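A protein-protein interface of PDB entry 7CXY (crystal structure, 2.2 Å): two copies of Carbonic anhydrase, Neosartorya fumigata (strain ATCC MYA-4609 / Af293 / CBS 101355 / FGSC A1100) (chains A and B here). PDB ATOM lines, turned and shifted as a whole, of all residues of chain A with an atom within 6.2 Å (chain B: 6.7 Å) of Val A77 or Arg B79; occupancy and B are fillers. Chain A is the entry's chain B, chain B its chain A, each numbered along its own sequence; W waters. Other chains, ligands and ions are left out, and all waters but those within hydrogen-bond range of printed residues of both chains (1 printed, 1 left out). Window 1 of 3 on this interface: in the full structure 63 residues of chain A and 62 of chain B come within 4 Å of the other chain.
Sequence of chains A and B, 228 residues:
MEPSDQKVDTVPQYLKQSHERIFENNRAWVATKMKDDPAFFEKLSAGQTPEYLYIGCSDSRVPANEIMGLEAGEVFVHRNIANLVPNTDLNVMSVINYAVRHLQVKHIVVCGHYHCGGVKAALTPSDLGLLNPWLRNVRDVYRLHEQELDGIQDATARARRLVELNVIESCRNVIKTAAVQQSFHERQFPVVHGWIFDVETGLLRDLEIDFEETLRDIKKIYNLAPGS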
ATOM      1  N   TYR A  52     -22.165   5.981  18.774  1.00  0.00           N
ATOM      2  CA  TYR A  52     -21.404   6.282  17.549  1.00  0.00           C
ATOM      3  C   TYR A  52     -19.898   6.079  17.646  1.00  0.00           C
ATOM      4  O   TYR A  52     -19.321   6.412  18.653  1.00  0.00           O
ATOM      5  CB  TYR A  52     -21.487   7.781  17.294  1.00  0.00           C
ATOM      6  CG  TYR A  52     -22.724   8.168  16.549  1.00  0.00           C
ATOM      7  CD1 TYR A  52     -23.933   8.313  17.200  1.00  0.00           C
ATOM      8  CD2 TYR A  52     -22.688   8.337  15.188  1.00  0.00           C
ATOM      9  CE1 TYR A  52     -25.086   8.616  16.508  1.00  0.00           C
ATOM     10  CE2 TYR A  52     -23.827   8.635  14.479  1.00  0.00           C
ATOM     11  CZ  TYR A  52     -25.023   8.787  15.144  1.00  0.00           C
ATOM     12  OH  TYR A  52     -26.129   9.097  14.427  1.00  0.00           O
ATOM     13  N   LEU A  53     -19.335   5.472  16.610  1.00  0.00           N
ATOM     14  CA  LEU A  53     -17.878   5.613  16.351  1.00  0.00           C
ATOM     15  C   LEU A  53     -17.692   6.707  15.308  1.00  0.00           C
ATOM     16  O   LEU A  53     -18.298   6.609  14.222  1.00  0.00           O
ATOM     17  CB  LEU A  53     -17.284   4.289  15.877  1.00  0.00           C
ATOM     18  CG  LEU A  53     -15.903   4.379  15.218  1.00  0.00           C
ATOM     19  CD1 LEU A  53     -14.852   4.965  16.160  1.00  0.00           C
ATOM     20  CD2 LEU A  53     -15.458   2.993  14.777  1.00  0.00           C
ATOM     21  N   TYR A  54     -16.880   7.706  15.628  1.00  0.00           N
ATOM     22  CA  TYR A  54     -16.510   8.804  14.720  1.00  0.00           C
ATOM     23  C   TYR A  54     -15.015   8.665  14.420  1.00  0.00           C
ATOM     24  O   TYR A  54     -14.174   8.644  15.356  1.00  0.00           O
ATOM     25  CB  TYR A  54     -16.879  10.133  15.366  1.00  0.00           C
ATOM     26  CG  TYR A  54     -16.422  11.389  14.667  1.00  0.00           C
ATOM     27  CD1 TYR A  54     -15.158  11.888  14.889  1.00  0.00           C
ATOM     28  CD2 TYR A  54     -17.280  12.151  13.899  1.00  0.00           C
ATOM     29  CE1 TYR A  54     -14.724  13.062  14.305  1.00  0.00           C
ATOM     30  CE2 TYR A  54     -16.858  13.322  13.299  1.00  0.00           C
ATOM     31  CZ  TYR A  54     -15.573  13.778  13.498  1.00  0.00           C
ATOM     32  OH  TYR A  54     -15.114  14.942  12.926  1.00  0.00           O
ATOM     33  N   ILE A  55     -14.698   8.571  13.131  1.00  0.00           N
ATOM     34  CA  ILE A  55     -13.315   8.608  12.612  1.00  0.00           C
ATOM     35  C   ILE A  55     -13.163   9.932  11.882  1.00  0.00           C
ATOM     36  O   ILE A  55     -13.851  10.153  10.898  1.00  0.00           O
ATOM     37  CB  ILE A  55     -13.006   7.390  11.735  1.00  0.00           C
ATOM     38  CG1 ILE A  55     -13.303   6.100  12.487  1.00  0.00           C
ATOM     39  CG2 ILE A  55     -11.567   7.463  11.267  1.00  0.00           C
ATOM     40  CD1 ILE A  55     -13.114   4.844  11.685  1.00  0.00           C
ATOM     41  N   GLY A  56     -12.300  10.792  12.399  1.00  0.00           N
ATOM     42  CA  GLY A  56     -12.066  12.125  11.846  1.00  0.00           C
ATOM     43  C   GLY A  56     -10.588  12.416  11.747  1.00  0.00           C
ATOM     44  O   GLY A  56      -9.759  11.506  11.952  1.00  0.00           O
ATOM     45  N   SER A  58      -7.066  14.452  12.616  1.00  0.00           N
ATOM     46  CA  SER A  58      -6.314  15.102  13.707  1.00  0.00           C
ATOM     47  C   SER A  58      -6.348  16.638  13.556  1.00  0.00           C
ATOM     48  O   SER A  58      -6.359  17.298  14.618  1.00  0.00           O
ATOM     49  CB  SER A  58      -4.899  14.535  13.765  1.00  0.00           C
ATOM     50  OG  SER A  58      -4.946  13.153  14.109  1.00  0.00           O
ATOM     51  N   PRO A  63     -14.646  19.430  17.906  1.00  0.00           N
ATOM     52  CA  PRO A  63     -14.878  18.041  18.295  1.00  0.00           C
ATOM     53  C   PRO A  63     -16.242  17.530  17.810  1.00  0.00           C
ATOM     54  O   PRO A  63     -17.177  18.293  17.676  1.00  0.00           O
ATOM     55  CB  PRO A  63     -14.799  18.081  19.824  1.00  0.00           C
ATOM     56  CG  PRO A  63     -15.211  19.497  20.164  1.00  0.00           C
ATOM     57  CD  PRO A  63     -14.639  20.351  19.052  1.00  0.00           C
ATOM     58  N   ALA A  64     -16.292  16.229  17.565  1.00  0.00           N
ATOM     59  CA  ALA A  64     -17.414  15.506  16.941  1.00  0.00           C
ATOM     60  C   ALA A  64     -18.716  15.837  17.676  1.00  0.00           C
ATOM     61  O   ALA A  64     -19.680  16.244  17.004  1.00  0.00           O
ATOM     62  CB  ALA A  64     -17.120  14.029  16.945  1.00  0.00           C
ATOM     63  N   VAL A  75     -20.103   9.571  21.849  1.00  0.00           N
ATOM     64  CA  VAL A  75     -19.210   9.332  20.676  1.00  0.00           C
ATOM     65  C   VAL A  75     -17.855   8.755  21.110  1.00  0.00           C
ATOM     66  O   VAL A  75     -17.110   9.422  21.825  1.00  0.00           O
ATOM     67  CB  VAL A  75     -19.032  10.603  19.847  1.00  0.00           C
ATOM     68  CG1 VAL A  75     -18.485  10.262  18.476  1.00  0.00           C
ATOM     69  CG2 VAL A  75     -20.329  11.373  19.689  1.00  0.00           C
ATOM     70  N   PHE A  76     -17.571   7.521  20.701  1.00  0.00           N
ATOM     71  CA  PHE A  76     -16.233   6.881  20.711  1.00  0.00           C
ATOM     72  C   PHE A  76     -15.447   7.463  19.531  1.00  0.00           C
ATOM     73  O   PHE A  76     -15.981   7.436  18.396  1.00  0.00           O
ATOM     74  CB  PHE A  76     -16.431   5.381  20.590  1.00  0.00           C
ATOM     75  CG  PHE A  76     -15.217   4.523  20.813  1.00  0.00           C
ATOM     76  CD1 PHE A  76     -14.642   4.408  22.066  1.00  0.00           C
ATOM     77  CD2 PHE A  76     -14.736   3.720  19.799  1.00  0.00           C
ATOM     78  CE1 PHE A  76     -13.553   3.575  22.267  1.00  0.00           C
ATOM     79  CE2 PHE A  76     -13.661   2.872  20.001  1.00  0.00           C
ATOM     80  CZ  PHE A  76     -13.070   2.810  21.239  1.00  0.00           C
ATOM     81  N   VAL A  77     -14.260   8.026  19.775  1.00  0.00           N
ATOM     82  CA  VAL A  77     -13.561   8.874  18.771  1.00  0.00           C
ATOM     83  C   VAL A  77     -12.190   8.303  18.414  1.00  0.00           C
ATOM     84  O   VAL A  77     -11.401   8.003  19.335  1.00  0.00           O
ATOM     85  CB  VAL A  77     -13.400  10.290  19.289  1.00  0.00           C
ATOM     86  CG1 VAL A  77     -12.634  11.155  18.302  1.00  0.00           C
ATOM     87  CG2 VAL A  77     -14.766  10.880  19.586  1.00  0.00           C
ATOM     88  N   HIS A  78     -11.894   8.270  17.112  1.00  0.00           N
ATOM     89  CA  HIS A  78     -10.537   8.096  16.561  1.00  0.00           C
ATOM     90  C   HIS A  78     -10.267   9.260  15.633  1.00  0.00           C
ATOM     91  O   HIS A  78     -11.106   9.574  14.806  1.00  0.00           O
ATOM     92  CB  HIS A  78     -10.364   6.732  15.902  1.00  0.00           C
ATOM     93  CG  HIS A  78      -9.024   6.517  15.296  1.00  0.00           C
ATOM     94  ND1 HIS A  78      -7.914   6.259  16.061  1.00  0.00           N
ATOM     95  CD2 HIS A  78      -8.602   6.481  14.007  1.00  0.00           C
ATOM     96  CE1 HIS A  78      -6.866   6.052  15.272  1.00  0.00           C
ATOM     97  NE2 HIS A  78      -7.247   6.190  14.012  1.00  0.00           N
ATOM     98  N   ARG A  79      -9.122   9.898  15.794  1.00  0.00           N
ATOM     99  CA  ARG A  79      -8.651  10.955  14.871  1.00  0.00           C
ATOM    100  C   ARG A  79      -7.243  10.578  14.421  1.00  0.00           C
ATOM    101  O   ARG A  79      -6.431  10.203  15.304  1.00  0.00           O
ATOM    102  CB  ARG A  79      -8.725  12.342  15.511  1.00  0.00           C
ATOM    103  CG  ARG A  79     -10.165  12.781  15.763  1.00  0.00           C
ATOM    104  CD  ARG A  79     -10.423  13.978  16.651  1.00  0.00           C
ATOM    105  NE  ARG A  79     -10.020  15.223  16.043  1.00  0.00           N
ATOM    106  CZ  ARG A  79     -10.083  16.414  16.651  1.00  0.00           C
ATOM    107  NH1 ARG A  79     -10.582  16.534  17.875  1.00  0.00           N
ATOM    108  NH2 ARG A  79      -9.651  17.494  16.014  1.00  0.00           N
ATOM    109  N   ASN A  80      -6.967  10.716  13.121  1.00  0.00           N
ATOM    110  CA  ASN A  80      -5.631  10.402  12.549  1.00  0.00           C
ATOM    111  C   ASN A  80      -5.396  11.370  11.394  1.00  0.00           C
ATOM    112  O   ASN A  80      -6.336  12.102  11.068  1.00  0.00           O
ATOM    113  CB  ASN A  80      -5.503   8.908  12.242  1.00  0.00           C
ATOM    114  CG  ASN A  80      -6.360   8.432  11.090  1.00  0.00           C
ATOM    115  OD1 ASN A  80      -6.459   9.145  10.095  1.00  0.00           O
ATOM    116  ND2 ASN A  80      -6.914   7.229  11.175  1.00  0.00           N
ATOM    117  N   ASN A  91      -3.935   0.229  14.640  1.00  0.00           N
ATOM    118  CA  ASN A  91      -4.461   1.338  15.460  1.00  0.00           C
ATOM    119  C   ASN A  91      -5.951   1.516  15.109  1.00  0.00           C
ATOM    120  O   ASN A  91      -6.812   1.233  15.981  1.00  0.00           O
ATOM    121  CB  ASN A  91      -3.571   2.554  15.279  1.00  0.00           C
ATOM    122  CG  ASN A  91      -3.943   3.698  16.181  1.00  0.00           C
ATOM    123  OD1 ASN A  91      -5.085   3.772  16.622  1.00  0.00           O
ATOM    124  ND2 ASN A  91      -3.011   4.620  16.388  1.00  0.00           N
ATOM    125  N   VAL A  95      -9.675   0.085  16.942  1.00  0.00           N
ATOM    126  CA  VAL A  95     -10.783   1.024  17.263  1.00  0.00           C
ATOM    127  C   VAL A  95     -12.098   0.431  16.725  1.00  0.00           C
ATOM    128  O   VAL A  95     -13.073   0.350  17.478  1.00  0.00           O
ATOM    129  CB  VAL A  95     -10.528   2.423  16.681  1.00  0.00           C
ATOM    130  CG1 VAL A  95     -11.797   3.260  16.658  1.00  0.00           C
ATOM    131  CG2 VAL A  95      -9.433   3.131  17.440  1.00  0.00           C
ATOM    132  N   TYR B  54      -2.223  16.586  21.293  1.00  0.00           N
ATOM    133  CA  TYR B  54      -2.859  15.851  22.399  1.00  0.00           C
ATOM    134  C   TYR B  54      -3.043  14.398  21.966  1.00  0.00           C
ATOM    135  O   TYR B  54      -3.642  14.147  20.946  1.00  0.00           O
ATOM    136  CB  TYR B  54      -4.176  16.534  22.764  1.00  0.00           C
ATOM    137  CG  TYR B  54      -5.049  15.836  23.771  1.00  0.00           C
ATOM    138  CD1 TYR B  54      -5.896  14.821  23.383  1.00  0.00           C
ATOM    139  CD2 TYR B  54      -5.050  16.199  25.101  1.00  0.00           C
ATOM    140  CE1 TYR B  54      -6.720  14.180  24.283  1.00  0.00           C
ATOM    141  CE2 TYR B  54      -5.867  15.573  26.020  1.00  0.00           C
ATOM    142  CZ  TYR B  54      -6.703  14.560  25.604  1.00  0.00           C
ATOM    143  OH  TYR B  54      -7.511  13.915  26.469  1.00  0.00           O
ATOM    144  N   ILE B  55      -2.512  13.483  22.750  1.00  0.00           N
ATOM    145  CA  ILE B  55      -2.726  12.039  22.501  1.00  0.00           C
ATOM    146  C   ILE B  55      -3.565  11.528  23.667  1.00  0.00           C
ATOM    147  O   ILE B  55      -3.108  11.574  24.797  1.00  0.00           O
ATOM    148  CB  ILE B  55      -1.402  11.291  22.321  1.00  0.00           C
ATOM    149  CG1 ILE B  55      -0.603  11.873  21.160  1.00  0.00           C
ATOM    150  CG2 ILE B  55      -1.649   9.812  22.158  1.00  0.00           C
ATOM    151  CD1 ILE B  55       0.795  11.376  21.085  1.00  0.00           C
ATOM    152  N   GLY B  56      -4.736  11.008  23.350  1.00  0.00           N
ATOM    153  CA  GLY B  56      -5.690  10.586  24.370  1.00  0.00           C
ATOM    154  C   GLY B  56      -6.381   9.306  24.008  1.00  0.00           C
ATOM    155  O   GLY B  56      -6.090   8.753  22.983  1.00  0.00           O
ATOM    156  N   CYS B  57      -7.179   8.809  24.927  1.00  0.00           N
ATOM    157  CA  CYS B  57      -7.930   7.569  24.700  1.00  0.00           C
ATOM    158  C   CYS B  57      -9.227   7.833  23.933  1.00  0.00           C
ATOM    159  O   CYS B  57      -9.870   8.801  24.184  1.00  0.00           O
ATOM    160  CB  CYS B  57      -8.245   6.916  26.027  1.00  0.00           C
ATOM    161  SG  CYS B  57      -9.043   5.316  25.852  1.00  0.00           S
ATOM    162  N   SER B  58      -9.590   6.893  23.082  1.00  0.00           N
ATOM    163  CA  SER B  58     -10.834   6.876  22.284  1.00  0.00           C
ATOM    164  C   SER B  58     -12.065   6.837  23.200  1.00  0.00           C
ATOM    165  O   SER B  58     -13.039   7.455  22.850  1.00  0.00           O
ATOM    166  CB  SER B  58     -10.806   5.708  21.344  1.00  0.00           C
ATOM    167  OG  SER B  58      -9.962   5.962  20.258  1.00  0.00           O
ATOM    168  N   ASP B  59     -11.981   6.149  24.339  1.00  0.00           N
ATOM    169  CA  ASP B  59     -13.127   5.914  25.271  1.00  0.00           C
ATOM    170  C   ASP B  59     -13.110   6.917  26.419  1.00  0.00           C
ATOM    171  O   ASP B  59     -13.937   6.733  27.340  1.00  0.00           O
ATOM    172  CB  ASP B  59     -13.261   4.478  25.818  1.00  0.00           C
ATOM    173  CG  ASP B  59     -12.179   3.947  26.755  1.00  0.00           C
ATOM    174  OD1 ASP B  59     -11.732   4.687  27.834  1.00  0.00           O
ATOM    175  OD2 ASP B  59     -11.709   2.849  26.594  1.00  0.00           O
ATOM    176  N   SER B  60     -12.247   7.931  26.372  1.00  0.00           N
ATOM    177  CA  SER B  60     -12.330   9.108  27.274  1.00  0.00           C
ATOM    178  C   SER B  60     -13.543   9.912  26.804  1.00  0.00           C
ATOM    179  O   SER B  60     -13.895   9.766  25.597  1.00  0.00           O
ATOM    180  CB  SER B  60     -11.040   9.914  27.350  1.00  0.00           C
ATOM    181  OG  SER B  60     -10.819  10.714  26.191  1.00  0.00           O
ATOM    182  N   ARG B  61     -14.147  10.681  27.728  1.00  0.00           N
ATOM    183  CA  ARG B  61     -15.581  11.088  27.704  1.00  0.00           C
ATOM    184  C   ARG B  61     -15.725  12.602  27.535  1.00  0.00           C
ATOM    185  O   ARG B  61     -16.873  13.080  27.517  1.00  0.00           O
ATOM    186  CB  ARG B  61     -16.281  10.695  29.008  1.00  0.00           C
ATOM    187  CG  ARG B  61     -16.475   9.198  29.192  1.00  0.00           C
ATOM    188  CD  ARG B  61     -16.861   8.810  30.608  1.00  0.00           C
ATOM    189  NE  ARG B  61     -16.102   7.658  31.106  1.00  0.00           N
ATOM    190  CZ  ARG B  61     -16.451   6.381  30.961  1.00  0.00           C
ATOM    191  NH1 ARG B  61     -15.672   5.431  31.453  1.00  0.00           N
ATOM    192  NH2 ARG B  61     -17.573   6.053  30.336  1.00  0.00           N
ATOM    193  N   VAL B  62     -14.613  13.332  27.462  1.00  0.00           N
ATOM    194  CA  VAL B  62     -14.611  14.807  27.252  1.00  0.00           C
ATOM    195  C   VAL B  62     -13.478  15.150  26.303  1.00  0.00           C
ATOM    196  O   VAL B  62     -12.344  14.740  26.515  1.00  0.00           O
ATOM    197  CB  VAL B  62     -14.478  15.584  28.574  1.00  0.00           C
ATOM    198  CG1 VAL B  62     -14.567  17.083  28.363  1.00  0.00           C
ATOM    199  CG2 VAL B  62     -15.512  15.140  29.584  1.00  0.00           C
ATOM    200  N   PRO B  63     -13.740  15.967  25.266  1.00  0.00           N
ATOM    201  CA  PRO B  63     -12.696  16.323  24.320  1.00  0.00           C
ATOM    202  C   PRO B  63     -11.635  17.209  24.978  1.00  0.00           C
ATOM    203  O   PRO B  63     -11.934  17.953  25.898  1.00  0.00           O
ATOM    204  CB  PRO B  63     -13.441  17.079  23.210  1.00  0.00           C
ATOM    205  CG  PRO B  63     -14.652  17.637  23.908  1.00  0.00           C
ATOM    206  CD  PRO B  63     -15.032  16.602  24.953  1.00  0.00           C
ATOM    207  N   ALA B  64     -10.429  17.106  24.440  1.00  0.00           N
ATOM    208  CA  ALA B  64      -9.190  17.741  24.932  1.00  0.00           C
ATOM    209  C   ALA B  64      -9.422  19.233  25.162  1.00  0.00           C
ATOM    210  O   ALA B  64      -9.156  19.712  26.275  1.00  0.00           O
ATOM    211  CB  ALA B  64      -8.114  17.521  23.905  1.00  0.00           C
ATOM    212  N   VAL B  77      -5.116  16.580  17.477  1.00  0.00           N
ATOM    213  CA  VAL B  77      -5.587  15.479  18.364  1.00  0.00           C
ATOM    214  C   VAL B  77      -5.368  14.113  17.715  1.00  0.00           C
ATOM    215  O   VAL B  77      -5.722  13.937  16.541  1.00  0.00           O
ATOM    216  CB  VAL B  77      -7.075  15.658  18.666  1.00  0.00           C
ATOM    217  CG1 VAL B  77      -7.615  14.522  19.519  1.00  0.00           C
ATOM    218  CG2 VAL B  77      -7.328  17.006  19.308  1.00  0.00           C
ATOM    219  N   HIS B  78      -4.878  13.164  18.501  1.00  0.00           N
ATOM    220  CA  HIS B  78      -4.912  11.716  18.210  1.00  0.00           C
ATOM    221  C   HIS B  78      -5.605  11.025  19.375  1.00  0.00           C
ATOM    222  O   HIS B  78      -5.246  11.285  20.507  1.00  0.00           O
ATOM    223  CB  HIS B  78      -3.526  11.166  17.889  1.00  0.00           C
ATOM    224  CG  HIS B  78      -3.516   9.697  17.605  1.00  0.00           C
ATOM    225  ND1 HIS B  78      -3.992   9.169  16.442  1.00  0.00           N
ATOM    226  CD2 HIS B  78      -3.083   8.642  18.332  1.00  0.00           C
ATOM    227  CE1 HIS B  78      -3.877   7.845  16.472  1.00  0.00           C
ATOM    228  NE2 HIS B  78      -3.309   7.498  17.604  1.00  0.00           N
ATOM    229  N   ARG B  79      -6.582  10.173  19.101  1.00  0.00           N
ATOM    230  CA  ARG B  79      -7.178   9.312  20.149  1.00  0.00           C
ATOM    231  C   ARG B  79      -7.156   7.873  19.664  1.00  0.00           C
ATOM    232  O   ARG B  79      -7.501   7.647  18.478  1.00  0.00           O
ATOM    233  CB  ARG B  79      -8.614   9.735  20.448  1.00  0.00           C
ATOM    234  CG  ARG B  79      -8.795  11.112  21.069  1.00  0.00           C
ATOM    235  CD  ARG B  79      -9.950  10.983  22.060  1.00  0.00           C
ATOM    236  NE  ARG B  79     -10.945  11.996  21.956  1.00  0.00           N
ATOM    237  CZ  ARG B  79     -12.161  11.947  22.511  1.00  0.00           C
ATOM    238  NH1 ARG B  79     -12.575  10.901  23.222  1.00  0.00           N
ATOM    239  NH2 ARG B  79     -12.975  12.971  22.316  1.00  0.00           N
ATOM    240  N   ASN B  80      -6.831   6.944  20.548  1.00  0.00           N
ATOM    241  CA  ASN B  80      -6.730   5.506  20.205  1.00  0.00           C
ATOM    242  C   ASN B  80      -7.092   4.703  21.452  1.00  0.00           C
ATOM    243  O   ASN B  80      -7.256   5.312  22.488  1.00  0.00           O
ATOM    244  CB  ASN B  80      -5.363   5.223  19.565  1.00  0.00           C
ATOM    245  CG  ASN B  80      -4.192   5.333  20.523  1.00  0.00           C
ATOM    246  OD1 ASN B  80      -4.305   4.926  21.676  1.00  0.00           O
ATOM    247  ND2 ASN B  80      -3.051   5.794  20.032  1.00  0.00           N
ATOM    248  N   ILE B  81      -7.226   3.387  21.378  1.00  0.00           N
ATOM    249  CA  ILE B  81      -7.597   2.569  22.561  1.00  0.00           C
ATOM    250  C   ILE B  81      -6.430   2.640  23.553  1.00  0.00           C
ATOM    251  O   ILE B  81      -5.318   2.118  23.220  1.00  0.00           O
ATOM    252  CB  ILE B  81      -7.898   1.093  22.239  1.00  0.00           C
ATOM    253  CG1 ILE B  81      -8.874   0.880  21.090  1.00  0.00           C
ATOM    254  CG2 ILE B  81      -8.326   0.363  23.505  1.00  0.00           C
ATOM    255  CD1 ILE B  81      -9.991   1.811  21.151  1.00  0.00           C
ATOM    256  N   ASN B  83      -4.731   5.186  24.804  1.00  0.00           N
ATOM    257  CA  ASN B  83      -3.758   6.308  24.609  1.00  0.00           C
ATOM    258  C   ASN B  83      -2.337   5.741  24.509  1.00  0.00           C
ATOM    259  O   ASN B  83      -1.449   6.189  25.227  1.00  0.00           O
ATOM    260  CB  ASN B  83      -3.893   7.416  25.668  1.00  0.00           C
ATOM    261  CG  ASN B  83      -3.988   6.906  27.104  1.00  0.00           C
ATOM    262  OD1 ASN B  83      -5.084   6.606  27.608  1.00  0.00           O
ATOM    263  ND2 ASN B  83      -2.851   6.774  27.769  1.00  0.00           N
HETATM  264  O   HOH W   1      -6.523   1.901  18.911  1.00  0.00           O
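Pro B63 touches its own counterpart, Pro A63.
His A78 touches its own counterpart, His B78.
His A78 touches Arg B79, and with the chains exchanged Arg A79 touches His B78.
Arg A79 touches its own counterpart, Arg B79.
Positions printed for both chains: 54, 55, 56, 58, 63, 64, 77, 78, 79 and 80.
Of the 15 pairs that touch across the chains among the printed residues, 9 have their exchanged pair printed and touching as well.
O of Val A77 lies within hydrogen-bond range of OG of Ser B58 (2.7 Å).
O of Val B77 is in hydrogen-bond range of OG of Ser A58, at 2.7 Å.
ND1 of His B78 lies within hydrogen-bond range of O of Arg A79 (2.9 Å).
ND2 of Asn A91 sits at hydrogen-bond distance from NE2 of His B78 (3.1 Å).
The backbone carbonyl oxygen (O) of Arg B79 sits at hydrogen-bond distance from a ring nitrogen (ND1) of His A78.
OG of Ser B58 sits close to O of Arg B79 (3.5 Å).
The backbone carbonyl oxygen of Ser B60 is in hydrogen-bond range of the guanidinium group of Arg B79, at 2.9 Å.
The backbone carbonyl oxygen of Tyr A52 lies within hydrogen-bond range of the backbone NH of Phe A76 (2.9 Å).
The backbone NH (N) of His A78 sits at hydrogen-bond distance from the backbone carbonyl oxygen (O) of Tyr A54 (2.9 Å).
The backbone NH (N) of Gly A56 is in hydrogen-bond range of the backbone carbonyl oxygen (O) of His A78, 3.0 Å away.
NE2 of His A78 lies within hydrogen-bond range of ND2 of Asn A80 (3.0 Å).
Among the printed residues, pairs that only touch across the chains: Pro A63 with Pro B63, Phe A76 with Ser B58, Phe A76 with Asp B59, Phe A76 with Ile B81, Val A77 with Arg B79, His A78 with His B78, Arg A79 with Val B77, Arg A79 with Arg B79, Asn A91 with Asn B80 and Val A95 with Ile B81.
Val A77 touches just these residues of chain B: Ser B58 (2.7 Å) and Arg B79 (3.5 Å).
Of chain A, only Val A77 (3.5 Å), His A78 (2.8 Å) and Arg A79 (3.8 Å) come within 4 Å of Arg B79.
Printed residues of chain B within 4 Å of Asn A91: His B78 (3.1 Å) and Asn B80 (3.3 Å).
Of the printed residues of chain B, His A78 touches His B78 and Arg B79.
Printed residues of chain B within 4 Å of Ser A58: Val B77.
Printed residues of chain A within 4 Å of His B78: His A78, Arg A79 and Asn A91.
Of the printed residues of chain B, Phe A76 touches Ser B58 (3.5 Å), Asp B59 (3.7 Å) and Ile B81 (3.2 Å).
Ser B60 touches none of the printed residues of chain A.
Ile A55 touches none of the printed residues of chain B.
The nearest printed residue of chain A that does not touch Ile B81 is Asn A91 (5.2 Å).
Hydrophobic or aromatic side chains of chain A that line the printed part of chain B: Pro A63, Phe A76, Val A77, His A78 and Val A95.
Of the 17 printed residues of chain B, 8 touch a printed residue of chain A.
Water W1 bridges N of Ile B81 and O of Asn A91.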
